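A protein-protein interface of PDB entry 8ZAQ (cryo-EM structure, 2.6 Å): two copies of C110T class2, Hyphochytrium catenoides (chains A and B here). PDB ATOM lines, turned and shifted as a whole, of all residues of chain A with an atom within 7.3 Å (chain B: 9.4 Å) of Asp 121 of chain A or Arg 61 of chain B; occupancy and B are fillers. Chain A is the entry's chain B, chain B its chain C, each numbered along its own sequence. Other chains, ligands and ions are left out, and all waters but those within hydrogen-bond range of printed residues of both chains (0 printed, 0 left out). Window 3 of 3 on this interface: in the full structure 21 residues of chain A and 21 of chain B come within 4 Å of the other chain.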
ATOM      1  N   ASP A 115      26.740   2.978  -8.551  1.00  0.00           N
ATOM      2  CA  ASP A 115      25.660   3.101  -9.518  1.00  0.00           C
ATOM      3  C   ASP A 115      24.327   2.770  -8.868  1.00  0.00           C
ATOM      4  O   ASP A 115      23.367   3.547  -8.960  1.00  0.00           O
ATOM      5  CB  ASP A 115      25.930   2.190 -10.716  1.00  0.00           C
ATOM      6  CG  ASP A 115      24.809   2.214 -11.731  1.00  0.00           C
ATOM      7  OD1 ASP A 115      24.598   3.270 -12.364  1.00  0.00           O
ATOM      8  OD2 ASP A 115      24.140   1.174 -11.900  1.00  0.00           O
ATOM      9  N   PHE A 116      24.272   1.648  -8.143  1.00  0.00           N
ATOM     10  CA  PHE A 116      23.044   1.285  -7.448  1.00  0.00           C
ATOM     11  C   PHE A 116      22.611   2.401  -6.513  1.00  0.00           C
ATOM     12  O   PHE A 116      21.462   2.860  -6.571  1.00  0.00           O
ATOM     13  CB  PHE A 116      23.250  -0.017  -6.676  1.00  0.00           C
ATOM     14  CG  PHE A 116      21.976  -0.728  -6.330  1.00  0.00           C
ATOM     15  CD1 PHE A 116      20.969  -0.869  -7.266  1.00  0.00           C
ATOM     16  CD2 PHE A 116      21.785  -1.253  -5.064  1.00  0.00           C
ATOM     17  CE1 PHE A 116      19.798  -1.525  -6.950  1.00  0.00           C
ATOM     18  CE2 PHE A 116      20.615  -1.910  -4.742  1.00  0.00           C
ATOM     19  CZ  PHE A 116      19.621  -2.045  -5.688  1.00  0.00           C
ATOM     20  N   ALA A 117      23.541   2.900  -5.694  1.00  0.00           N
ATOM     21  CA  ALA A 117      23.203   3.955  -4.751  1.00  0.00           C
ATOM     22  C   ALA A 117      22.719   5.202  -5.470  1.00  0.00           C
ATOM     23  O   ALA A 117      21.876   5.932  -4.941  1.00  0.00           O
ATOM     24  CB  ALA A 117      24.406   4.278  -3.869  1.00  0.00           C
ATOM     25  N   PHE A 118      23.226   5.455  -6.679  1.00  0.00           N
ATOM     26  CA  PHE A 118      22.775   6.620  -7.421  1.00  0.00           C
ATOM     27  C   PHE A 118      21.411   6.390  -8.051  1.00  0.00           C
ATOM     28  O   PHE A 118      20.629   7.338  -8.187  1.00  0.00           O
ATOM     29  CB  PHE A 118      23.802   6.995  -8.489  1.00  0.00           C
ATOM     30  CG  PHE A 118      24.899   7.884  -7.981  1.00  0.00           C
ATOM     31  CD1 PHE A 118      24.607   9.118  -7.429  1.00  0.00           C
ATOM     32  CD2 PHE A 118      26.221   7.487  -8.055  1.00  0.00           C
ATOM     33  CE1 PHE A 118      25.612   9.936  -6.961  1.00  0.00           C
ATOM     34  CE2 PHE A 118      27.230   8.301  -7.588  1.00  0.00           C
ATOM     35  CZ  PHE A 118      26.925   9.527  -7.041  1.00  0.00           C
ATOM     36  N   THR A 119      21.101   5.150  -8.430  1.00  0.00           N
ATOM     37  CA  THR A 119      19.825   4.885  -9.081  1.00  0.00           C
ATOM     38  C   THR A 119      18.671   4.893  -8.089  1.00  0.00           C
ATOM     39  O   THR A 119      17.558   5.297  -8.441  1.00  0.00           O
ATOM     40  CB  THR A 119      19.877   3.547  -9.821  1.00  0.00           C
ATOM     41  OG1 THR A 119      21.120   3.441 -10.525  1.00  0.00           O
ATOM     42  CG2 THR A 119      18.734   3.436 -10.813  1.00  0.00           C
ATOM     43  N   LEU A 120      18.917   4.462  -6.853  1.00  0.00           N
ATOM     44  CA  LEU A 120      17.886   4.379  -5.829  1.00  0.00           C
ATOM     45  C   LEU A 120      17.955   5.522  -4.828  1.00  0.00           C
ATOM     46  O   LEU A 120      17.155   5.553  -3.888  1.00  0.00           O
ATOM     47  CB  LEU A 120      17.984   3.038  -5.099  1.00  0.00           C
ATOM     48  CG  LEU A 120      17.021   1.944  -5.552  1.00  0.00           C
ATOM     49  CD1 LEU A 120      17.300   1.550  -6.989  1.00  0.00           C
ATOM     50  CD2 LEU A 120      17.133   0.744  -4.631  1.00  0.00           C
ATOM     51  N   ASP A 121      18.879   6.464  -5.012  1.00  0.00           N
ATOM     52  CA  ASP A 121      19.094   7.569  -4.080  1.00  0.00           C
ATOM     53  C   ASP A 121      19.308   7.043  -2.660  1.00  0.00           C
ATOM     54  O   ASP A 121      18.724   7.520  -1.686  1.00  0.00           O
ATOM     55  CB  ASP A 121      17.937   8.569  -4.135  1.00  0.00           C
ATOM     56  CG  ASP A 121      18.284   9.897  -3.493  1.00  0.00           C
ATOM     57  OD1 ASP A 121      19.477  10.264  -3.489  1.00  0.00           O
ATOM     58  OD2 ASP A 121      17.365  10.575  -2.989  1.00  0.00           O
ATOM     59  N   LEU A 122      20.156   6.028  -2.566  1.00  0.00           N
ATOM     60  CA  LEU A 122      20.454   5.421  -1.279  1.00  0.00           C
ATOM     61  C   LEU A 122      21.397   6.314  -0.479  1.00  0.00           C
ATOM     62  O   LEU A 122      22.294   6.939  -1.052  1.00  0.00           O
ATOM     63  CB  LEU A 122      21.084   4.047  -1.470  1.00  0.00           C
ATOM     64  CG  LEU A 122      20.167   3.020  -2.137  1.00  0.00           C
ATOM     65  CD1 LEU A 122      20.942   1.781  -2.536  1.00  0.00           C
ATOM     66  CD2 LEU A 122      19.008   2.659  -1.228  1.00  0.00           C
ATOM     67  N   PRO A 123      21.209   6.401   0.834  1.00  0.00           N
ATOM     68  CA  PRO A 123      22.108   7.219   1.653  1.00  0.00           C
ATOM     69  C   PRO A 123      23.468   6.561   1.817  1.00  0.00           C
ATOM     70  O   PRO A 123      23.640   5.359   1.602  1.00  0.00           O
ATOM     71  CB  PRO A 123      21.375   7.317   2.994  1.00  0.00           C
ATOM     72  CG  PRO A 123      20.522   6.109   3.039  1.00  0.00           C
ATOM     73  CD  PRO A 123      20.114   5.818   1.626  1.00  0.00           C
ATOM     74  N   HIS A 124      24.444   7.383   2.203  1.00  0.00           N
ATOM     75  CA  HIS A 124      25.795   6.919   2.524  1.00  0.00           C
ATOM     76  C   HIS A 124      26.429   6.192   1.340  1.00  0.00           C
ATOM     77  O   HIS A 124      26.869   5.046   1.447  1.00  0.00           O
ATOM     78  CB  HIS A 124      25.791   6.034   3.772  1.00  0.00           C
ATOM     79  CG  HIS A 124      24.813   6.469   4.818  1.00  0.00           C
ATOM     80  ND1 HIS A 124      23.836   5.635   5.314  1.00  0.00           N
ATOM     81  CD2 HIS A 124      24.664   7.650   5.463  1.00  0.00           C
ATOM     82  CE1 HIS A 124      23.124   6.284   6.218  1.00  0.00           C
ATOM     83  NE2 HIS A 124      23.607   7.509   6.327  1.00  0.00           N
ATOM     84  N   LYS A 125      26.474   6.877   0.197  1.00  0.00           N
ATOM     85  CA  LYS A 125      27.064   6.285  -0.999  1.00  0.00           C
ATOM     86  C   LYS A 125      28.552   6.017  -0.811  1.00  0.00           C
ATOM     87  O   LYS A 125      29.060   4.972  -1.233  1.00  0.00           O
ATOM     88  CB  LYS A 125      26.825   7.196  -2.201  1.00  0.00           C
ATOM     89  CG  LYS A 125      25.363   7.543  -2.422  1.00  0.00           C
ATOM     90  CD  LYS A 125      25.139   8.166  -3.786  1.00  0.00           C
ATOM     91  CE  LYS A 125      23.671   8.461  -4.017  1.00  0.00           C
ATOM     92  NZ  LYS A 125      22.977   8.848  -2.764  1.00  0.00           N
ATOM     93  N   HIS A 171      18.069  -0.262   3.609  1.00  0.00           N
ATOM     94  CA  HIS A 171      17.851   0.964   2.855  1.00  0.00           C
ATOM     95  C   HIS A 171      17.070   0.683   1.582  1.00  0.00           C
ATOM     96  O   HIS A 171      16.187   1.462   1.204  1.00  0.00           O
ATOM     97  CB  HIS A 171      19.186   1.636   2.541  1.00  0.00           C
ATOM     98  CG  HIS A 171      19.781   2.361   3.707  1.00  0.00           C
ATOM     99  ND1 HIS A 171      21.137   2.562   3.847  1.00  0.00           N
ATOM    100  CD2 HIS A 171      19.203   2.929   4.792  1.00  0.00           C
ATOM    101  CE1 HIS A 171      21.368   3.224   4.966  1.00  0.00           C
ATOM    102  NE2 HIS A 171      20.212   3.460   5.557  1.00  0.00           N
ATOM    103  N   ARG A 175      13.540   2.359   0.094  1.00  0.00           N
ATOM    104  CA  ARG A 175      13.325   2.932  -1.226  1.00  0.00           C
ATOM    105  C   ARG A 175      12.276   2.162  -2.014  1.00  0.00           C
ATOM    106  O   ARG A 175      11.613   2.740  -2.882  1.00  0.00           O
ATOM    107  CB  ARG A 175      14.642   2.972  -2.001  1.00  0.00           C
ATOM    108  CG  ARG A 175      15.613   4.018  -1.496  1.00  0.00           C
ATOM    109  CD  ARG A 175      14.977   5.395  -1.478  1.00  0.00           C
ATOM    110  NE  ARG A 175      14.927   5.990  -2.808  1.00  0.00           N
ATOM    111  CZ  ARG A 175      14.363   7.157  -3.083  1.00  0.00           C
ATOM    112  NH1 ARG A 175      13.784   7.883  -2.143  1.00  0.00           N
ATOM    113  NH2 ARG A 175      14.381   7.607  -4.334  1.00  0.00           N
ATOM    114  N   TYR A 179       8.839   3.647  -5.059  1.00  0.00           N
ATOM    115  CA  TYR A 179       8.708   3.566  -6.504  1.00  0.00           C
ATOM    116  C   TYR A 179       7.388   2.912  -6.914  1.00  0.00           C
ATOM    117  O   TYR A 179       6.795   2.152  -6.145  1.00  0.00           O
ATOM    118  CB  TYR A 179       9.886   2.794  -7.082  1.00  0.00           C
ATOM    119  CG  TYR A 179      11.201   3.487  -6.818  1.00  0.00           C
ATOM    120  CD1 TYR A 179      11.439   4.765  -7.297  1.00  0.00           C
ATOM    121  CD2 TYR A 179      12.190   2.880  -6.057  1.00  0.00           C
ATOM    122  CE1 TYR A 179      12.631   5.409  -7.049  1.00  0.00           C
ATOM    123  CE2 TYR A 179      13.387   3.520  -5.804  1.00  0.00           C
ATOM    124  CZ  TYR A 179      13.601   4.784  -6.304  1.00  0.00           C
ATOM    125  OH  TYR A 179      14.786   5.430  -6.057  1.00  0.00           O
ATOM    126  N   PHE A 242      14.807  -0.244 -15.063  1.00  0.00           N
ATOM    127  CA  PHE A 242      14.222   0.432 -13.911  1.00  0.00           C
ATOM    128  C   PHE A 242      14.323   1.944 -14.054  1.00  0.00           C
ATOM    129  O   PHE A 242      13.372   2.666 -13.742  1.00  0.00           O
ATOM    130  CB  PHE A 242      14.909  -0.039 -12.627  1.00  0.00           C
ATOM    131  CG  PHE A 242      14.626   0.826 -11.432  1.00  0.00           C
ATOM    132  CD1 PHE A 242      13.473   0.648 -10.690  1.00  0.00           C
ATOM    133  CD2 PHE A 242      15.516   1.813 -11.045  1.00  0.00           C
ATOM    134  CE1 PHE A 242      13.211   1.439  -9.591  1.00  0.00           C
ATOM    135  CE2 PHE A 242      15.256   2.606  -9.951  1.00  0.00           C
ATOM    136  CZ  PHE A 242      14.104   2.418  -9.223  1.00  0.00           C
ATOM    137  N   GLU A 259       6.407   8.774  -1.997  1.00  0.00           N
ATOM    138  CA  GLU A 259       7.286   9.125  -0.891  1.00  0.00           C
ATOM    139  C   GLU A 259       6.561   9.984   0.141  1.00  0.00           C
ATOM    140  O   GLU A 259       5.339  10.128   0.096  1.00  0.00           O
ATOM    141  CB  GLU A 259       8.524   9.857  -1.412  1.00  0.00           C
ATOM    142  CG  GLU A 259       9.777   9.623  -0.590  1.00  0.00           C
ATOM    143  CD  GLU A 259      11.037   9.629  -1.433  1.00  0.00           C
ATOM    144  OE1 GLU A 259      12.035   9.005  -1.016  1.00  0.00           O
ATOM    145  OE2 GLU A 259      11.029  10.253  -2.515  1.00  0.00           O
ATOM    146  N   LEU B  46      27.634  10.828  13.609  1.00  0.00           N
ATOM    147  CA  LEU B  46      27.221  11.590  12.439  1.00  0.00           C
ATOM    148  C   LEU B  46      25.777  11.284  12.064  1.00  0.00           C
ATOM    149  O   LEU B  46      25.017  12.188  11.700  1.00  0.00           O
ATOM    150  CB  LEU B  46      28.161  11.289  11.276  1.00  0.00           C
ATOM    151  CG  LEU B  46      27.842  11.973   9.958  1.00  0.00           C
ATOM    152  CD1 LEU B  46      28.102  13.459  10.078  1.00  0.00           C
ATOM    153  CD2 LEU B  46      28.673  11.361   8.854  1.00  0.00           C
ATOM    154  N   ASP B  47      25.379  10.015  12.144  1.00  0.00           N
ATOM    155  CA  ASP B  47      24.005   9.642  11.838  1.00  0.00           C
ATOM    156  C   ASP B  47      23.012  10.076  12.908  1.00  0.00           C
ATOM    157  O   ASP B  47      21.803  10.020  12.664  1.00  0.00           O
ATOM    158  CB  ASP B  47      23.899   8.129  11.632  1.00  0.00           C
ATOM    159  CG  ASP B  47      24.565   7.670  10.354  1.00  0.00           C
ATOM    160  OD1 ASP B  47      24.737   8.503   9.440  1.00  0.00           O
ATOM    161  OD2 ASP B  47      24.909   6.474  10.259  1.00  0.00           O
ATOM    162  N   LEU B  48      23.481  10.504  14.076  1.00  0.00           N
ATOM    163  CA  LEU B  48      22.591  10.915  15.153  1.00  0.00           C
ATOM    164  C   LEU B  48      21.900  12.233  14.823  1.00  0.00           C
ATOM    165  O   LEU B  48      20.963  12.640  15.507  1.00  0.00           O
ATOM    166  CB  LEU B  48      23.360  11.046  16.470  1.00  0.00           C
ATOM    167  CG  LEU B  48      23.594   9.773  17.284  1.00  0.00           C
ATOM    168  CD1 LEU B  48      23.944  10.121  18.720  1.00  0.00           C
ATOM    169  CD2 LEU B  48      22.384   8.861  17.236  1.00  0.00           C
ATOM    170  N   MET B  50      22.714  16.828  13.794  1.00  0.00           N
ATOM    171  CA  MET B  50      23.654  17.940  13.759  1.00  0.00           C
ATOM    172  C   MET B  50      23.874  18.538  15.142  1.00  0.00           C
ATOM    173  O   MET B  50      22.924  18.897  15.832  1.00  0.00           O
ATOM    174  CB  MET B  50      23.166  19.027  12.800  1.00  0.00           C
ATOM    175  CG  MET B  50      23.464  18.747  11.340  1.00  0.00           C
ATOM    176  SD  MET B  50      22.364  19.617  10.208  1.00  0.00           S
ATOM    177  CE  MET B  50      20.844  19.637  11.148  1.00  0.00           C
ATOM    178  N   LYS B  55      20.147  17.590  16.180  1.00  0.00           N
ATOM    179  CA  LYS B  55      19.053  18.096  15.364  1.00  0.00           C
ATOM    180  C   LYS B  55      18.934  17.260  14.095  1.00  0.00           C
ATOM    181  O   LYS B  55      19.934  17.065  13.393  1.00  0.00           O
ATOM    182  CB  LYS B  55      19.284  19.564  15.018  1.00  0.00           C
ATOM    183  CG  LYS B  55      18.085  20.259  14.396  1.00  0.00           C
ATOM    184  CD  LYS B  55      18.523  21.321  13.407  1.00  0.00           C
ATOM    185  CE  LYS B  55      17.952  22.681  13.765  1.00  0.00           C
ATOM    186  NZ  LYS B  55      17.695  23.504  12.554  1.00  0.00           N
ATOM    187  N   PRO B  56      17.750  16.740  13.778  1.00  0.00           N
ATOM    188  CA  PRO B  56      17.615  15.881  12.595  1.00  0.00           C
ATOM    189  C   PRO B  56      17.958  16.624  11.313  1.00  0.00           C
ATOM    190  O   PRO B  56      17.672  17.813  11.163  1.00  0.00           O
ATOM    191  CB  PRO B  56      16.140  15.465  12.624  1.00  0.00           C
ATOM    192  CG  PRO B  56      15.469  16.463  13.505  1.00  0.00           C
ATOM    193  CD  PRO B  56      16.484  16.876  14.515  1.00  0.00           C
ATOM    194  N   TYR B  57      18.583  15.905  10.387  1.00  0.00           N
ATOM    195  CA  TYR B  57      18.898  16.473   9.085  1.00  0.00           C
ATOM    196  C   TYR B  57      17.619  16.742   8.305  1.00  0.00           C
ATOM    197  O   TYR B  57      16.650  15.980   8.386  1.00  0.00           O
ATOM    198  CB  TYR B  57      19.804  15.527   8.299  1.00  0.00           C
ATOM    199  CG  TYR B  57      21.134  15.258   8.964  1.00  0.00           C
ATOM    200  CD1 TYR B  57      22.208  16.115   8.783  1.00  0.00           C
ATOM    201  CD2 TYR B  57      21.314  14.144   9.772  1.00  0.00           C
ATOM    202  CE1 TYR B  57      23.422  15.872   9.388  1.00  0.00           C
ATOM    203  CE2 TYR B  57      22.527  13.894  10.381  1.00  0.00           C
ATOM    204  CZ  TYR B  57      23.576  14.762  10.186  1.00  0.00           C
ATOM    205  OH  TYR B  57      24.788  14.520  10.789  1.00  0.00           O
ATOM    206  N   LYS B  58      17.614  17.843   7.550  1.00  0.00           N
ATOM    207  CA  LYS B  58      16.443  18.176   6.747  1.00  0.00           C
ATOM    208  C   LYS B  58      16.179  17.113   5.690  1.00  0.00           C
ATOM    209  O   LYS B  58      15.025  16.736   5.453  1.00  0.00           O
ATOM    210  CB  LYS B  58      16.624  19.547   6.097  1.00  0.00           C
ATOM    211  CG  LYS B  58      16.222  20.709   6.988  1.00  0.00           C
ATOM    212  CD  LYS B  58      14.851  20.485   7.606  1.00  0.00           C
ATOM    213  CE  LYS B  58      14.715  21.229   8.924  1.00  0.00           C
ATOM    214  NZ  LYS B  58      15.896  21.017   9.807  1.00  0.00           N
ATOM    215  N   SER B  59      17.234  16.613   5.049  1.00  0.00           N
ATOM    216  CA  SER B  59      17.096  15.552   4.061  1.00  0.00           C
ATOM    217  C   SER B  59      17.054  14.164   4.685  1.00  0.00           C
ATOM    218  O   SER B  59      16.878  13.182   3.957  1.00  0.00           O
ATOM    219  CB  SER B  59      18.241  15.631   3.049  1.00  0.00           C
ATOM    220  OG  SER B  59      19.289  14.745   3.393  1.00  0.00           O
ATOM    221  N   GLY B  60      17.213  14.058   6.002  1.00  0.00           N
ATOM    222  CA  GLY B  60      17.189  12.784   6.684  1.00  0.00           C
ATOM    223  C   GLY B  60      18.506  12.042   6.702  1.00  0.00           C
ATOM    224  O   GLY B  60      18.595  10.988   7.343  1.00  0.00           O
ATOM    225  N   ARG B  61      19.528  12.554   6.024  1.00  0.00           N
ATOM    226  CA  ARG B  61      20.831  11.913   5.973  1.00  0.00           C
ATOM    227  C   ARG B  61      21.913  12.975   6.070  1.00  0.00           C
ATOM    228  O   ARG B  61      21.713  14.126   5.675  1.00  0.00           O
ATOM    229  CB  ARG B  61      21.007  11.094   4.687  1.00  0.00           C
ATOM    230  CG  ARG B  61      20.470  11.784   3.448  1.00  0.00           C
ATOM    231  CD  ARG B  61      20.648  10.935   2.207  1.00  0.00           C
ATOM    232  NE  ARG B  61      19.478  10.110   1.934  1.00  0.00           N
ATOM    233  CZ  ARG B  61      19.227   9.537   0.766  1.00  0.00           C
ATOM    234  NH1 ARG B  61      20.038   9.688  -0.267  1.00  0.00           N
ATOM    235  NH2 ARG B  61      18.132   8.795   0.630  1.00  0.00           N
ATOM    236  N   ALA B  62      23.060  12.577   6.601  1.00  0.00           N
ATOM    237  CA  ALA B  62      24.191  13.474   6.742  1.00  0.00           C
ATOM    238  C   ALA B  62      24.849  13.730   5.390  1.00  0.00           C
ATOM    239  O   ALA B  62      24.685  12.948   4.451  1.00  0.00           O
ATOM    240  CB  ALA B  62      25.205  12.885   7.714  1.00  0.00           C
ATOM    241  N   PRO B  63      25.585  14.835   5.258  1.00  0.00           N
ATOM    242  CA  PRO B  63      26.378  15.043   4.042  1.00  0.00           C
ATOM    243  C   PRO B  63      27.389  13.923   3.852  1.00  0.00           C
ATOM    244  O   PRO B  63      27.965  13.411   4.812  1.00  0.00           O
ATOM    245  CB  PRO B  63      27.064  16.389   4.294  1.00  0.00           C
ATOM    246  CG  PRO B  63      26.169  17.088   5.252  1.00  0.00           C
ATOM    247  CD  PRO B  63      25.599  16.018   6.136  1.00  0.00           C
ATOM    248  N   GLU B  64      27.597  13.544   2.590  1.00  0.00           N
ATOM    249  CA  GLU B  64      28.435  12.388   2.293  1.00  0.00           C
ATOM    250  C   GLU B  64      29.891  12.620   2.675  1.00  0.00           C
ATOM    251  O   GLU B  64      30.563  11.689   3.129  1.00  0.00           O
ATOM    252  CB  GLU B  64      28.324  12.026   0.814  1.00  0.00           C
ATOM    253  CG  GLU B  64      26.897  11.835   0.345  1.00  0.00           C
ATOM    254  CD  GLU B  64      26.532  10.377   0.174  1.00  0.00           C
ATOM    255  OE1 GLU B  64      27.402   9.516   0.413  1.00  0.00           O
ATOM    256  OE2 GLU B  64      25.374  10.091  -0.194  1.00  0.00           O
ATOM    257  N   VAL B  65      30.399  13.845   2.496  1.00  0.00           N
ATOM    258  CA  VAL B  65      31.776  14.151   2.864  1.00  0.00           C
ATOM    259  C   VAL B  65      31.985  14.157   4.370  1.00  0.00           C
ATOM    260  O   VAL B  65      33.126  14.011   4.828  1.00  0.00           O
ATOM    261  CB  VAL B  65      32.222  15.506   2.280  1.00  0.00           C
ATOM    262  CG1 VAL B  65      32.538  15.361   0.803  1.00  0.00           C
ATOM    263  CG2 VAL B  65      31.157  16.559   2.510  1.00  0.00           C
ATOM    264  N   ASN B  66      30.923  14.321   5.154  1.00  0.00           N
ATOM    265  CA  ASN B  66      31.015  14.267   6.604  1.00  0.00           C
ATOM    266  C   ASN B  66      31.340  12.875   7.123  1.00  0.00           C
ATOM    267  O   ASN B  66      31.775  12.743   8.271  1.00  0.00           O
ATOM    268  CB  ASN B  66      29.708  14.752   7.235  1.00  0.00           C
ATOM    269  CG  ASN B  66      29.544  16.250   7.150  1.00  0.00           C
ATOM    270  OD1 ASN B  66      29.833  16.861   6.124  1.00  0.00           O
ATOM    271  ND2 ASN B  66      29.074  16.853   8.232  1.00  0.00           N
ATOM    272  N   SER B  67      31.141  11.842   6.309  1.00  0.00           N
ATOM    273  CA  SER B  67      31.492  10.478   6.675  1.00  0.00           C
ATOM    274  C   SER B  67      32.961  10.168   6.444  1.00  0.00           C
ATOM    275  O   SER B  67      33.398   9.058   6.758  1.00  0.00           O
ATOM    276  CB  SER B  67      30.637   9.483   5.886  1.00  0.00           C
ATOM    277  OG  SER B  67      29.321   9.973   5.706  1.00  0.00           O
ATOM    278  N   GLU B 247      28.040  22.756  14.168  1.00  0.00           N
ATOM    279  CA  GLU B 247      26.632  22.543  13.870  1.00  0.00           C
ATOM    280  C   GLU B 247      25.741  23.074  14.983  1.00  0.00           C
ATOM    281  O   GLU B 247      24.646  23.572  14.713  1.00  0.00           O
ATOM    282  CB  GLU B 247      26.367  21.055  13.637  1.00  0.00           C
ATOM    283  CG  GLU B 247      26.930  20.518  12.334  1.00  0.00           C
ATOM    284  CD  GLU B 247      27.105  19.011  12.352  1.00  0.00           C
ATOM    285  OE1 GLU B 247      27.211  18.434  13.453  1.00  0.00           O
ATOM    286  OE2 GLU B 247      27.146  18.401  11.264  1.00  0.00           O
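The side-chain carboxylate of Asp 121 of chain A lies within salt-bridge range of the guanidinium group of Arg 61 of chain B, at 3.3 Å. A ring nitrogen (NE2) of His 124 of chain A lies within hydrogen-bond range of the side-chain carboxylate (OD1) of Asp 47 of chain B, 3.5 Å away. NZ of Lys 125 of chain A lies within salt-bridge range of OE2 of Glu 64 of chain B (3.7 Å).
The side-chain carboxylate of Asp 121 of chain A is in salt-bridge range of the side-chain amino group of Lys 125 of chain A (3.8 Å). The backbone carbonyl oxygen (O) of Ala 117 of chain A is in hydrogen-bond range of the backbone NH (N) of Leu 122 of chain A. The backbone carbonyl oxygen of Glu 64 of chain B lies within hydrogen-bond range of the side-chain hydroxyl of Ser 67 of chain B (3.3 Å). The side-chain hydroxyl (OG) of Ser 59 of chain B sits close to the backbone carbonyl oxygen (O) of Arg 61 of chain B (3.4 Å). The backbone carbonyl oxygen (O) of Leu 122 of chain A lies within hydrogen-bond range of the side-chain amino group (NZ) of Lys 125 of chain A, 2.7 Å away.
Among the printed residues, pairs that only touch across the chains: Pro 123 of chain A with Arg 61 of chain B (3.5 Å), His 124 of chain A with Glu 64 of chain B (3.6 Å), Leu 122 of chain A with Arg 61 of chain B (3.6 Å) and Lys 125 of chain A with Arg 61 of chain B (3.9 Å).
Of chain B, only Arg 61 comes within 4 Å of Asp 121 of chain A. Arg 61 of chain B touches just these residues of chain A: Asp 121, Leu 122, Pro 123 and Lys 125. Of the printed residues of chain B, Lys 125 of chain A touches Arg 61 and Glu 64. Printed residues of chain A within 4 Å of Asp 47 of chain B: His 124 (3.5 Å). Tyr 179 of chain A touches none of the printed residues of chain B. Phe 242 of chain A touches none of the printed residues of chain B. The nearest printed residue of chain B that does not touch His 124 of chain A is Arg 61 of chain B (4.7 Å).
Of the 18 printed residues of chain B, 3 touch a printed residue of chain A. Hydrophobic or aromatic side chains of chain A that line the printed part of chain B: Pro 123 and His 124.
No position is printed for both chains.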
